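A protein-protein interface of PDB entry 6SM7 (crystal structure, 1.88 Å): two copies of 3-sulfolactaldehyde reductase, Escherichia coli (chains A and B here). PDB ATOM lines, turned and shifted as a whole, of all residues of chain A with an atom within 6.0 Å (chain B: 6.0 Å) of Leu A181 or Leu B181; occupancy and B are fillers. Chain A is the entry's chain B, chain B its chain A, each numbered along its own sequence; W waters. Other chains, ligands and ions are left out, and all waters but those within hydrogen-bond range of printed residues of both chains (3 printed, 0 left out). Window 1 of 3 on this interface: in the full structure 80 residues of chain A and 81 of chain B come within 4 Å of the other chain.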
ATOM      1  N   TYR A 176      -4.954  26.138  23.311  1.00  0.00           N
ATOM      2  CA  TYR A 176      -5.100  26.193  21.836  1.00  0.00           C
ATOM      3  C   TYR A 176      -6.582  25.993  21.500  1.00  0.00           C
ATOM      4  O   TYR A 176      -7.214  26.828  20.823  1.00  0.00           O
ATOM      5  CB  TYR A 176      -4.210  25.194  21.110  1.00  0.00           C
ATOM      6  CG  TYR A 176      -4.545  25.182  19.644  1.00  0.00           C
ATOM      7  CD1 TYR A 176      -4.353  26.300  18.870  1.00  0.00           C
ATOM      8  CD2 TYR A 176      -5.146  24.094  19.062  1.00  0.00           C
ATOM      9  CE1 TYR A 176      -4.688  26.319  17.533  1.00  0.00           C
ATOM     10  CE2 TYR A 176      -5.500  24.095  17.726  1.00  0.00           C
ATOM     11  CZ  TYR A 176      -5.302  25.226  16.961  1.00  0.00           C
ATOM     12  OH  TYR A 176      -5.643  25.217  15.632  1.00  0.00           O
ATOM     13  N   MET A 177      -7.144  24.892  21.981  1.00  0.00           N
ATOM     14  CA  MET A 177      -8.551  24.514  21.690  1.00  0.00           C
ATOM     15  C   MET A 177      -9.506  25.608  22.196  1.00  0.00           C
ATOM     16  O   MET A 177     -10.338  26.075  21.423  1.00  0.00           O
ATOM     17  CB  MET A 177      -8.893  23.152  22.317  1.00  0.00           C
ATOM     18  CG  MET A 177     -10.292  22.709  22.030  1.00  0.00           C
ATOM     19  SD  MET A 177     -10.450  22.268  20.279  1.00  0.00           S
ATOM     20  CE  MET A 177     -12.220  22.252  20.082  1.00  0.00           C
ATOM     21  N   SER A 178      -9.411  26.045  23.451  1.00  0.00           N
ATOM     22  CA  SER A 178     -10.391  27.016  23.993  1.00  0.00           C
ATOM     23  C   SER A 178     -10.244  28.354  23.256  1.00  0.00           C
ATOM     24  O   SER A 178     -11.275  28.979  22.952  1.00  0.00           O
ATOM     25  CB  SER A 178     -10.316  27.217  25.505  1.00  0.00           C
ATOM     26  OG  SER A 178      -9.045  27.729  25.865  1.00  0.00           O
ATOM     27  N   ILE A 179      -9.024  28.808  23.009  1.00  0.00           N
ATOM     28  CA  ILE A 179      -8.828  30.165  22.421  1.00  0.00           C
ATOM     29  C   ILE A 179      -9.358  30.164  20.973  1.00  0.00           C
ATOM     30  O   ILE A 179     -10.091  31.095  20.615  1.00  0.00           O
ATOM     31  CB  ILE A 179      -7.350  30.574  22.509  1.00  0.00           C
ATOM     32  CG1 ILE A 179      -6.865  30.696  23.960  1.00  0.00           C
ATOM     33  CG2 ILE A 179      -7.129  31.867  21.736  1.00  0.00           C
ATOM     34  CD1 ILE A 179      -5.346  30.742  24.066  1.00  0.00           C
ATOM     35  N   ALA A 180      -9.004  29.151  20.165  1.00  0.00           N
ATOM     36  CA  ALA A 180      -9.516  29.042  18.779  1.00  0.00           C
ATOM     37  C   ALA A 180     -11.042  28.850  18.812  1.00  0.00           C
ATOM     38  O   ALA A 180     -11.726  29.469  18.002  1.00  0.00           O
ATOM     39  CB  ALA A 180      -8.790  27.948  18.042  1.00  0.00           C
ATOM     40  N   LEU A 181     -11.569  28.065  19.763  1.00  0.00           N
ATOM     41  CA  LEU A 181     -13.026  27.765  19.840  1.00  0.00           C
ATOM     42  C   LEU A 181     -13.812  29.054  20.055  1.00  0.00           C
ATOM     43  O   LEU A 181     -14.914  29.207  19.520  1.00  0.00           O
ATOM     44  CB  LEU A 181     -13.273  26.769  20.974  1.00  0.00           C
ATOM     45  CG  LEU A 181     -14.732  26.430  21.235  1.00  0.00           C
ATOM     46  CD1 LEU A 181     -15.363  25.872  19.980  1.00  0.00           C
ATOM     47  CD2 LEU A 181     -14.844  25.453  22.410  1.00  0.00           C
ATOM     48  N   ASN A 182     -13.250  29.982  20.819  1.00  0.00           N
ATOM     49  CA  ASN A 182     -13.879  31.296  21.077  1.00  0.00           C
ATOM     50  C   ASN A 182     -14.128  32.024  19.744  1.00  0.00           C
ATOM     51  O   ASN A 182     -15.213  32.598  19.573  1.00  0.00           O
ATOM     52  CB  ASN A 182     -12.986  32.109  22.020  1.00  0.00           C
ATOM     53  CG  ASN A 182     -13.609  33.392  22.512  1.00  0.00           C
ATOM     54  OD1 ASN A 182     -14.801  33.447  22.816  1.00  0.00           O
ATOM     55  ND2 ASN A 182     -12.791  34.443  22.570  1.00  0.00           N
ATOM     56  N   ALA A 183     -13.148  32.038  18.842  1.00  0.00           N
ATOM     57  CA  ALA A 183     -13.272  32.725  17.544  1.00  0.00           C
ATOM     58  C   ALA A 183     -14.353  32.015  16.717  1.00  0.00           C
ATOM     59  O   ALA A 183     -15.158  32.703  16.059  1.00  0.00           O
ATOM     60  CB  ALA A 183     -11.947  32.751  16.831  1.00  0.00           C
ATOM     61  N   LEU A 184     -14.400  30.686  16.764  1.00  0.00           N
ATOM     62  CA  LEU A 184     -15.421  29.938  15.969  1.00  0.00           C
ATOM     63  C   LEU A 184     -16.801  30.208  16.564  1.00  0.00           C
ATOM     64  O   LEU A 184     -17.748  30.451  15.797  1.00  0.00           O
ATOM     65  CB  LEU A 184     -15.102  28.451  15.949  1.00  0.00           C
ATOM     66  CG  LEU A 184     -16.231  27.609  15.344  1.00  0.00           C
ATOM     67  CD1 LEU A 184     -16.504  28.014  13.896  1.00  0.00           C
ATOM     68  CD2 LEU A 184     -15.850  26.135  15.357  1.00  0.00           C
ATOM     69  N   SER A 185     -16.904  30.182  17.901  1.00  0.00           N
ATOM     70  CA  SER A 185     -18.149  30.443  18.646  1.00  0.00           C
ATOM     71  C   SER A 185     -18.720  31.800  18.242  1.00  0.00           C
ATOM     72  O   SER A 185     -19.937  31.900  17.988  1.00  0.00           O
ATOM     73  CB  SER A 185     -17.916  30.356  20.123  1.00  0.00           C
ATOM     74  OG  SER A 185     -17.479  29.066  20.471  1.00  0.00           O
ATOM     75  N   ALA A 186     -17.863  32.806  18.115  1.00  0.00           N
ATOM     76  CA  ALA A 186     -18.264  34.171  17.734  1.00  0.00           C
ATOM     77  C   ALA A 186     -18.847  34.167  16.326  1.00  0.00           C
ATOM     78  O   ALA A 186     -19.908  34.793  16.129  1.00  0.00           O
ATOM     79  CB  ALA A 186     -17.067  35.121  17.822  1.00  0.00           C
ATOM     80  N   ALA A 210     -23.128  17.998  19.393  1.00  0.00           N
ATOM     81  CA  ALA A 210     -21.672  18.235  19.402  1.00  0.00           C
ATOM     82  C   ALA A 210     -21.391  19.742  19.363  1.00  0.00           C
ATOM     83  O   ALA A 210     -20.296  20.131  19.790  1.00  0.00           O
ATOM     84  CB  ALA A 210     -21.005  17.503  18.272  1.00  0.00           C
ATOM     85  N   ALA A 211     -22.306  20.561  18.821  1.00  0.00           N
ATOM     86  CA  ALA A 211     -22.102  22.016  18.689  1.00  0.00           C
ATOM     87  C   ALA A 211     -21.769  22.597  20.069  1.00  0.00           C
ATOM     88  O   ALA A 211     -20.766  23.380  20.163  1.00  0.00           O
ATOM     89  CB  ALA A 211     -23.310  22.676  18.119  1.00  0.00           C
ATOM     90  N   GLY A 212     -22.534  22.191  21.092  1.00  0.00           N
ATOM     91  CA  GLY A 212     -22.410  22.714  22.474  1.00  0.00           C
ATOM     92  C   GLY A 212     -21.631  21.775  23.384  1.00  0.00           C
ATOM     93  O   GLY A 212     -21.055  22.253  24.360  1.00  0.00           O
ATOM     94  N   LYS A 213     -21.587  20.477  23.087  1.00  0.00           N
ATOM     95  CA  LYS A 213     -20.966  19.456  23.987  1.00  0.00           C
ATOM     96  C   LYS A 213     -19.579  19.074  23.501  1.00  0.00           C
ATOM     97  O   LYS A 213     -18.854  18.461  24.257  1.00  0.00           O
ATOM     98  CB  LYS A 213     -21.848  18.209  24.098  1.00  0.00           C
ATOM     99  CG  LYS A 213     -23.192  18.439  24.785  1.00  0.00           C
ATOM    100  CD  LYS A 213     -23.947  17.161  25.068  1.00  0.00           C
ATOM    101  CE  LYS A 213     -24.468  16.504  23.815  1.00  0.00           C
ATOM    102  NZ  LYS A 213     -25.495  15.485  24.150  1.00  0.00           N
ATOM    103  N   GLY A 214     -19.218  19.402  22.258  1.00  0.00           N
ATOM    104  CA  GLY A 214     -17.929  18.965  21.693  1.00  0.00           C
ATOM    105  C   GLY A 214     -18.024  17.574  21.076  1.00  0.00           C
ATOM    106  O   GLY A 214     -18.965  16.843  21.404  1.00  0.00           O
ATOM    107  N   HIS A 215     -17.093  17.258  20.187  1.00  0.00           N
ATOM    108  CA  HIS A 215     -16.971  15.977  19.455  1.00  0.00           C
ATOM    109  C   HIS A 215     -16.193  14.943  20.281  1.00  0.00           C
ATOM    110  O   HIS A 215     -16.420  13.733  20.081  1.00  0.00           O
ATOM    111  CB  HIS A 215     -16.277  16.209  18.128  1.00  0.00           C
ATOM    112  CG  HIS A 215     -17.144  16.932  17.153  1.00  0.00           C
ATOM    113  ND1 HIS A 215     -18.082  16.271  16.355  1.00  0.00           N
ATOM    114  CD2 HIS A 215     -17.218  18.241  16.846  1.00  0.00           C
ATOM    115  CE1 HIS A 215     -18.702  17.167  15.617  1.00  0.00           C
ATOM    116  NE2 HIS A 215     -18.192  18.390  15.903  1.00  0.00           N
ATOM    117  N   LEU A 258     -12.837  31.133  10.084  1.00  0.00           N
ATOM    118  CA  LEU A 258     -12.613  29.748  10.552  1.00  0.00           C
ATOM    119  C   LEU A 258     -13.517  28.787   9.774  1.00  0.00           C
ATOM    120  O   LEU A 258     -13.040  27.699   9.397  1.00  0.00           O
ATOM    121  CB  LEU A 258     -12.798  29.625  12.062  1.00  0.00           C
ATOM    122  CG  LEU A 258     -11.555  29.928  12.896  1.00  0.00           C
ATOM    123  CD1 LEU A 258     -11.259  31.412  12.881  1.00  0.00           C
ATOM    124  CD2 LEU A 258     -11.742  29.430  14.327  1.00  0.00           C
ATOM    125  N   TYR B 176     -23.507  24.416  11.389  1.00  0.00           N
ATOM    126  CA  TYR B 176     -22.308  25.239  11.107  1.00  0.00           C
ATOM    127  C   TYR B 176     -21.305  25.027  12.249  1.00  0.00           C
ATOM    128  O   TYR B 176     -20.119  24.667  12.040  1.00  0.00           O
ATOM    129  CB  TYR B 176     -22.640  26.720  10.945  1.00  0.00           C
ATOM    130  CG  TYR B 176     -21.373  27.526  10.850  1.00  0.00           C
ATOM    131  CD1 TYR B 176     -20.474  27.318   9.819  1.00  0.00           C
ATOM    132  CD2 TYR B 176     -21.009  28.395  11.857  1.00  0.00           C
ATOM    133  CE1 TYR B 176     -19.270  27.996   9.766  1.00  0.00           C
ATOM    134  CE2 TYR B 176     -19.800  29.062  11.833  1.00  0.00           C
ATOM    135  CZ  TYR B 176     -18.926  28.869  10.781  1.00  0.00           C
ATOM    136  OH  TYR B 176     -17.709  29.493  10.743  1.00  0.00           O
ATOM    137  N   MET B 177     -21.767  25.243  13.471  1.00  0.00           N
ATOM    138  CA  MET B 177     -20.900  25.167  14.677  1.00  0.00           C
ATOM    139  C   MET B 177     -20.334  23.755  14.812  1.00  0.00           C
ATOM    140  O   MET B 177     -19.109  23.627  14.937  1.00  0.00           O
ATOM    141  CB  MET B 177     -21.699  25.552  15.927  1.00  0.00           C
ATOM    142  CG  MET B 177     -20.865  25.556  17.143  1.00  0.00           C
ATOM    143  SD  MET B 177     -19.647  26.927  17.108  1.00  0.00           S
ATOM    144  CE  MET B 177     -18.592  26.370  18.434  1.00  0.00           C
ATOM    145  N   SER B 178     -21.153  22.697  14.771  1.00  0.00           N
ATOM    146  CA  SER B 178     -20.619  21.334  14.989  1.00  0.00           C
ATOM    147  C   SER B 178     -19.662  20.963  13.855  1.00  0.00           C
ATOM    148  O   SER B 178     -18.636  20.353  14.133  1.00  0.00           O
ATOM    149  CB  SER B 178     -21.707  20.281  15.170  1.00  0.00           C
ATOM    150  OG  SER B 178     -22.492  20.195  14.015  1.00  0.00           O
ATOM    151  N   ILE B 179     -20.004  21.270  12.599  1.00  0.00           N
ATOM    152  CA  ILE B 179     -19.164  20.810  11.457  1.00  0.00           C
ATOM    153  C   ILE B 179     -17.788  21.513  11.513  1.00  0.00           C
ATOM    154  O   ILE B 179     -16.759  20.840  11.382  1.00  0.00           O
ATOM    155  CB  ILE B 179     -19.919  21.025  10.142  1.00  0.00           C
ATOM    156  CG1 ILE B 179     -21.193  20.171  10.068  1.00  0.00           C
ATOM    157  CG2 ILE B 179     -18.986  20.768   8.962  1.00  0.00           C
ATOM    158  CD1 ILE B 179     -22.151  20.567   9.007  1.00  0.00           C
ATOM    159  N   ALA B 180     -17.766  22.839  11.710  1.00  0.00           N
ATOM    160  CA  ALA B 180     -16.505  23.595  11.833  1.00  0.00           C
ATOM    161  C   ALA B 180     -15.746  23.125  13.089  1.00  0.00           C
ATOM    162  O   ALA B 180     -14.501  22.985  13.029  1.00  0.00           O
ATOM    163  CB  ALA B 180     -16.785  25.074  11.828  1.00  0.00           C
ATOM    164  N   LEU B 181     -16.449  22.872  14.194  1.00  0.00           N
ATOM    165  CA  LEU B 181     -15.809  22.507  15.487  1.00  0.00           C
ATOM    166  C   LEU B 181     -15.041  21.203  15.321  1.00  0.00           C
ATOM    167  O   LEU B 181     -13.947  21.026  15.920  1.00  0.00           O
ATOM    168  CB  LEU B 181     -16.887  22.355  16.554  1.00  0.00           C
ATOM    169  CG  LEU B 181     -16.430  21.887  17.927  1.00  0.00           C
ATOM    170  CD1 LEU B 181     -15.331  22.774  18.470  1.00  0.00           C
ATOM    171  CD2 LEU B 181     -17.634  21.884  18.847  1.00  0.00           C
ATOM    172  N   ASN B 182     -15.578  20.300  14.505  1.00  0.00           N
ATOM    173  CA  ASN B 182     -14.938  19.001  14.229  1.00  0.00           C
ATOM    174  C   ASN B 182     -13.540  19.234  13.649  1.00  0.00           C
ATOM    175  O   ASN B 182     -12.600  18.543  14.062  1.00  0.00           O
ATOM    176  CB  ASN B 182     -15.881  18.195  13.328  1.00  0.00           C
ATOM    177  CG  ASN B 182     -15.457  16.776  13.092  1.00  0.00           C
ATOM    178  OD1 ASN B 182     -14.996  16.110  14.018  1.00  0.00           O
ATOM    179  ND2 ASN B 182     -15.619  16.317  11.847  1.00  0.00           N
ATOM    180  N   ALA B 183     -13.394  20.157  12.694  1.00  0.00           N
ATOM    181  CA  ALA B 183     -12.093  20.441  12.053  1.00  0.00           C
ATOM    182  C   ALA B 183     -11.133  21.037  13.082  1.00  0.00           C
ATOM    183  O   ALA B 183      -9.938  20.648  13.090  1.00  0.00           O
ATOM    184  CB  ALA B 183     -12.252  21.346  10.858  1.00  0.00           C
ATOM    185  N   LEU B 184     -11.621  21.894  13.962  1.00  0.00           N
ATOM    186  CA  LEU B 184     -10.740  22.500  14.991  1.00  0.00           C
ATOM    187  C   LEU B 184     -10.327  21.433  16.008  1.00  0.00           C
ATOM    188  O   LEU B 184      -9.150  21.400  16.380  1.00  0.00           O
ATOM    189  CB  LEU B 184     -11.459  23.654  15.681  1.00  0.00           C
ATOM    190  CG  LEU B 184     -10.680  24.214  16.861  1.00  0.00           C
ATOM    191  CD1 LEU B 184      -9.356  24.761  16.385  1.00  0.00           C
ATOM    192  CD2 LEU B 184     -11.489  25.244  17.612  1.00  0.00           C
ATOM    193  N   SER B 185     -11.275  20.591  16.425  1.00  0.00           N
ATOM    194  CA  SER B 185     -11.057  19.477  17.382  1.00  0.00           C
ATOM    195  C   SER B 185      -9.938  18.582  16.851  1.00  0.00           C
ATOM    196  O   SER B 185      -9.029  18.207  17.628  1.00  0.00           O
ATOM    197  CB  SER B 185     -12.319  18.704  17.597  1.00  0.00           C
ATOM    198  OG  SER B 185     -13.323  19.527  18.118  1.00  0.00           O
ATOM    199  N   ALA B 186      -9.959  18.288  15.545  1.00  0.00           N
ATOM    200  CA  ALA B 186      -8.944  17.452  14.892  1.00  0.00           C
ATOM    201  C   ALA B 186      -7.566  18.114  15.020  1.00  0.00           C
ATOM    202  O   ALA B 186      -6.575  17.418  15.325  1.00  0.00           O
ATOM    203  CB  ALA B 186      -9.344  17.200  13.448  1.00  0.00           C
ATOM    204  N   ALA B 210     -13.485  25.648  28.969  1.00  0.00           N
ATOM    205  CA  ALA B 210     -14.247  26.034  27.762  1.00  0.00           C
ATOM    206  C   ALA B 210     -13.813  25.144  26.580  1.00  0.00           C
ATOM    207  O   ALA B 210     -14.594  25.050  25.637  1.00  0.00           O
ATOM    208  CB  ALA B 210     -14.073  27.511  27.479  1.00  0.00           C
ATOM    209  N   ALA B 211     -12.601  24.573  26.600  1.00  0.00           N
ATOM    210  CA  ALA B 211     -12.082  23.732  25.502  1.00  0.00           C
ATOM    211  C   ALA B 211     -13.094  22.611  25.206  1.00  0.00           C
ATOM    212  O   ALA B 211     -13.392  22.368  24.025  1.00  0.00           O
ATOM    213  CB  ALA B 211     -10.742  23.171  25.860  1.00  0.00           C
ATOM    214  N   GLY B 212     -13.596  21.958  26.264  1.00  0.00           N
ATOM    215  CA  GLY B 212     -14.510  20.799  26.182  1.00  0.00           C
ATOM    216  C   GLY B 212     -15.959  21.179  26.458  1.00  0.00           C
ATOM    217  O   GLY B 212     -16.856  20.466  25.973  1.00  0.00           O
ATOM    218  N   LYS B 213     -16.217  22.270  27.177  1.00  0.00           N
ATOM    219  CA  LYS B 213     -17.591  22.657  27.597  1.00  0.00           C
ATOM    220  C   LYS B 213     -18.153  23.743  26.693  1.00  0.00           C
ATOM    221  O   LYS B 213     -19.361  23.963  26.742  1.00  0.00           O
ATOM    222  CB  LYS B 213     -17.614  23.136  29.053  1.00  0.00           C
ATOM    223  CG  LYS B 213     -17.347  22.034  30.073  1.00  0.00           C
ATOM    224  CD  LYS B 213     -17.583  22.454  31.507  1.00  0.00           C
ATOM    225  CE  LYS B 213     -16.556  23.457  31.983  1.00  0.00           C
ATOM    226  N   GLY B 214     -17.314  24.413  25.892  1.00  0.00           N
ATOM    227  CA  GLY B 214     -17.806  25.538  25.070  1.00  0.00           C
ATOM    228  C   GLY B 214     -17.787  26.844  25.852  1.00  0.00           C
ATOM    229  O   GLY B 214     -17.752  26.801  27.105  1.00  0.00           O
ATOM    230  N   HIS B 215     -17.799  27.968  25.137  1.00  0.00           N
ATOM    231  CA  HIS B 215     -17.810  29.349  25.685  1.00  0.00           C
ATOM    232  C   HIS B 215     -19.236  29.815  25.931  1.00  0.00           C
ATOM    233  O   HIS B 215     -19.427  30.715  26.787  1.00  0.00           O
ATOM    234  CB  HIS B 215     -17.084  30.300  24.717  1.00  0.00           C
ATOM    235  CG  HIS B 215     -15.618  30.060  24.685  1.00  0.00           C
ATOM    236  ND1 HIS B 215     -14.761  30.652  25.591  1.00  0.00           N
ATOM    237  CD2 HIS B 215     -14.854  29.289  23.873  1.00  0.00           C
ATOM    238  CE1 HIS B 215     -13.534  30.245  25.349  1.00  0.00           C
ATOM    239  NE2 HIS B 215     -13.567  29.400  24.290  1.00  0.00           N
ATOM    240  N   LEU B 258      -7.341  26.302  10.926  1.00  0.00           N
ATOM    241  CA  LEU B 258      -8.346  27.042  11.735  1.00  0.00           C
ATOM    242  C   LEU B 258      -7.610  27.832  12.836  1.00  0.00           C
ATOM    243  O   LEU B 258      -7.986  28.977  13.088  1.00  0.00           O
ATOM    244  CB  LEU B 258      -9.413  26.114  12.323  1.00  0.00           C
ATOM    245  CG  LEU B 258     -10.595  25.835  11.394  1.00  0.00           C
ATOM    246  CD1 LEU B 258     -10.193  24.918  10.235  1.00  0.00           C
ATOM    247  CD2 LEU B 258     -11.750  25.258  12.186  1.00  0.00           C
HETATM  248  O   HOH W   1     -14.435  33.713  26.009  1.00  0.00           O
HETATM  249  O   HOH W   2     -14.984  19.102  20.272  1.00  0.00           O
HETATM  250  O   HOH W   3     -18.382  27.376  22.488  1.00  0.00           O
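A ring nitrogen (NE2) of His A215 lies within hydrogen-bond range of the backbone carbonyl oxygen (O) of Ser B178 (2.7 Å). The backbone carbonyl oxygen (O) of Gly A212 sits close to the backbone carbonyl oxygen (O) of Lys B213, 3.4 Å away. O of Lys A213 sits close to O of Gly B212, 3.3 Å away. A ring nitrogen (NE2) of His B215 sits at hydrogen-bond distance from the backbone carbonyl oxygen (O) of Ser A178.
O of Leu B181 sits at hydrogen-bond distance from OG of Ser B185, at 2.7 Å. O of Leu A181 is in hydrogen-bond range of OG of Ser A185 (2.7 Å).
Among the printed residues, pairs that only touch across the chains: Leu A181 with Ala B210 (3.3 Å), Ala A210 with Leu B181 (3.3 Å), Leu A181 with Leu B181 (3.4 Å), His A215 with Asn B182 (3.5 Å), Leu A184 with Leu B181 (3.5 Å), Asn A182 with His B215 (3.5 Å), Met A177 with Ser B185 (3.5 Å), Met A177 with Leu B181 (3.5 Å), Leu A181 with Leu B184 (3.5 Å), Ser A185 with Met B177 (3.6 Å), Leu A184 with Ala B180 (3.6 Å), Leu A181 with Met B177 (3.6 Å), Ala A180 with Leu B184 (3.6 Å), Ser A178 with Ala B211 (3.7 Å), Leu A258 with Leu B258 (3.7 Å), Leu A184 with Tyr B176 (3.7 Å), Met A177 with Ala B211 (3.7 Å), Ala A211 with Ser B178 (3.7 Å), Ala A211 with Leu B181 (3.7 Å), Ala A211 with Met B177 (3.7 Å), Leu A181 with Ala B211 (3.8 Å), Tyr A176 with Leu B184 (3.8 Å), His A215 with Leu B181 (3.9 Å), Leu A181 with His B215 (3.9 Å), Leu A184 with Met B177 (3.9 Å), Met A177 with Leu B184 (3.9 Å) and Leu A181 with Gly B214 (3.98 Å).
Printed residues of chain B within 4 Å of Ser A178: Ala B211 (3.7 Å) and His B215 (2.7 Å). Printed residues of chain B within 4 Å of Leu A181: Met B177 (3.6 Å), Leu B181 (3.4 Å), Leu B184 (3.5 Å), Ala B210 (3.3 Å), Ala B211 (3.8 Å), Gly B214 (3.98 Å) and His B215 (3.9 Å). Printed residues of chain B within 4 Å of Leu A184: Tyr B176 (3.7 Å), Met B177 (3.9 Å), Ala B180 (3.6 Å) and Leu B181 (3.5 Å). Printed residues of chain B within 4 Å of Leu A258: Leu B258 (3.7 Å). Printed residues of chain A within 4 Å of Met B177: Leu A181, Leu A184, Ser A185 and Ala A211. Leu B181 touches just these residues of chain A: Met A177, Leu A181, Leu A184, Ala A210, Ala A211 and His A215. Ala B183 touches none of the printed residues of chain A. Printed residues of chain A within 4 Å of Leu B258: Leu A258 (3.7 Å). The nearest printed residue of chain B that does not touch Leu A181 is Gly B212 (5.4 Å). The nearest residue of chain A that does not touch Leu B181 is Gly A214 (4.1 Å). The nearest printed residue of chain A that does not touch Ala B211 is Gly A214 (6.1 Å).
Hydrophobic or aromatic side chains of chain B that line the printed part of chain A: Tyr B176, Met B177, Ala B180, Leu B181, Leu B184, Ala B211, His B215 and Leu B258. Of the 18 printed residues of chain A, 14 touch a printed residue of chain B. Printed residues of chain A that touch a printed residue of chain B: Tyr A176, Met A177, Ser A178, Ala A180, Leu A181, Asn A182, Leu A184, Ser A185, Ala A210, Ala A211, Gly A212, Lys A213, His A215 and Leu A258. Among the printed residues, 31 pairs touch across the chains.
Met A177 touches Leu B184, and with the chains exchanged Leu A184 touches Met B177. Leu A181 touches Ala B210, and with the chains exchanged Ala A210 touches Leu B181. Leu A181 touches Gly B214, but with the chains exchanged Gly A214 does not touch Leu B181 (4.1 Å). Asn A182 touches His B215, and with the chains exchanged His A215 touches Asn B182.
Water W2 lies within hydrogen-bond range of the side-chain hydroxyl (OG) of Ser B185 (2.8 Å) and the backbone NH (N) of His A215 (2.8 Å). Water W3 bridges the backbone NH of His B215 (2.8 Å) and the side-chain hydroxyl of Ser A185 (2.8 Å). Water W1 bridges ND1 of His B215 and OD1 of Asn A182.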
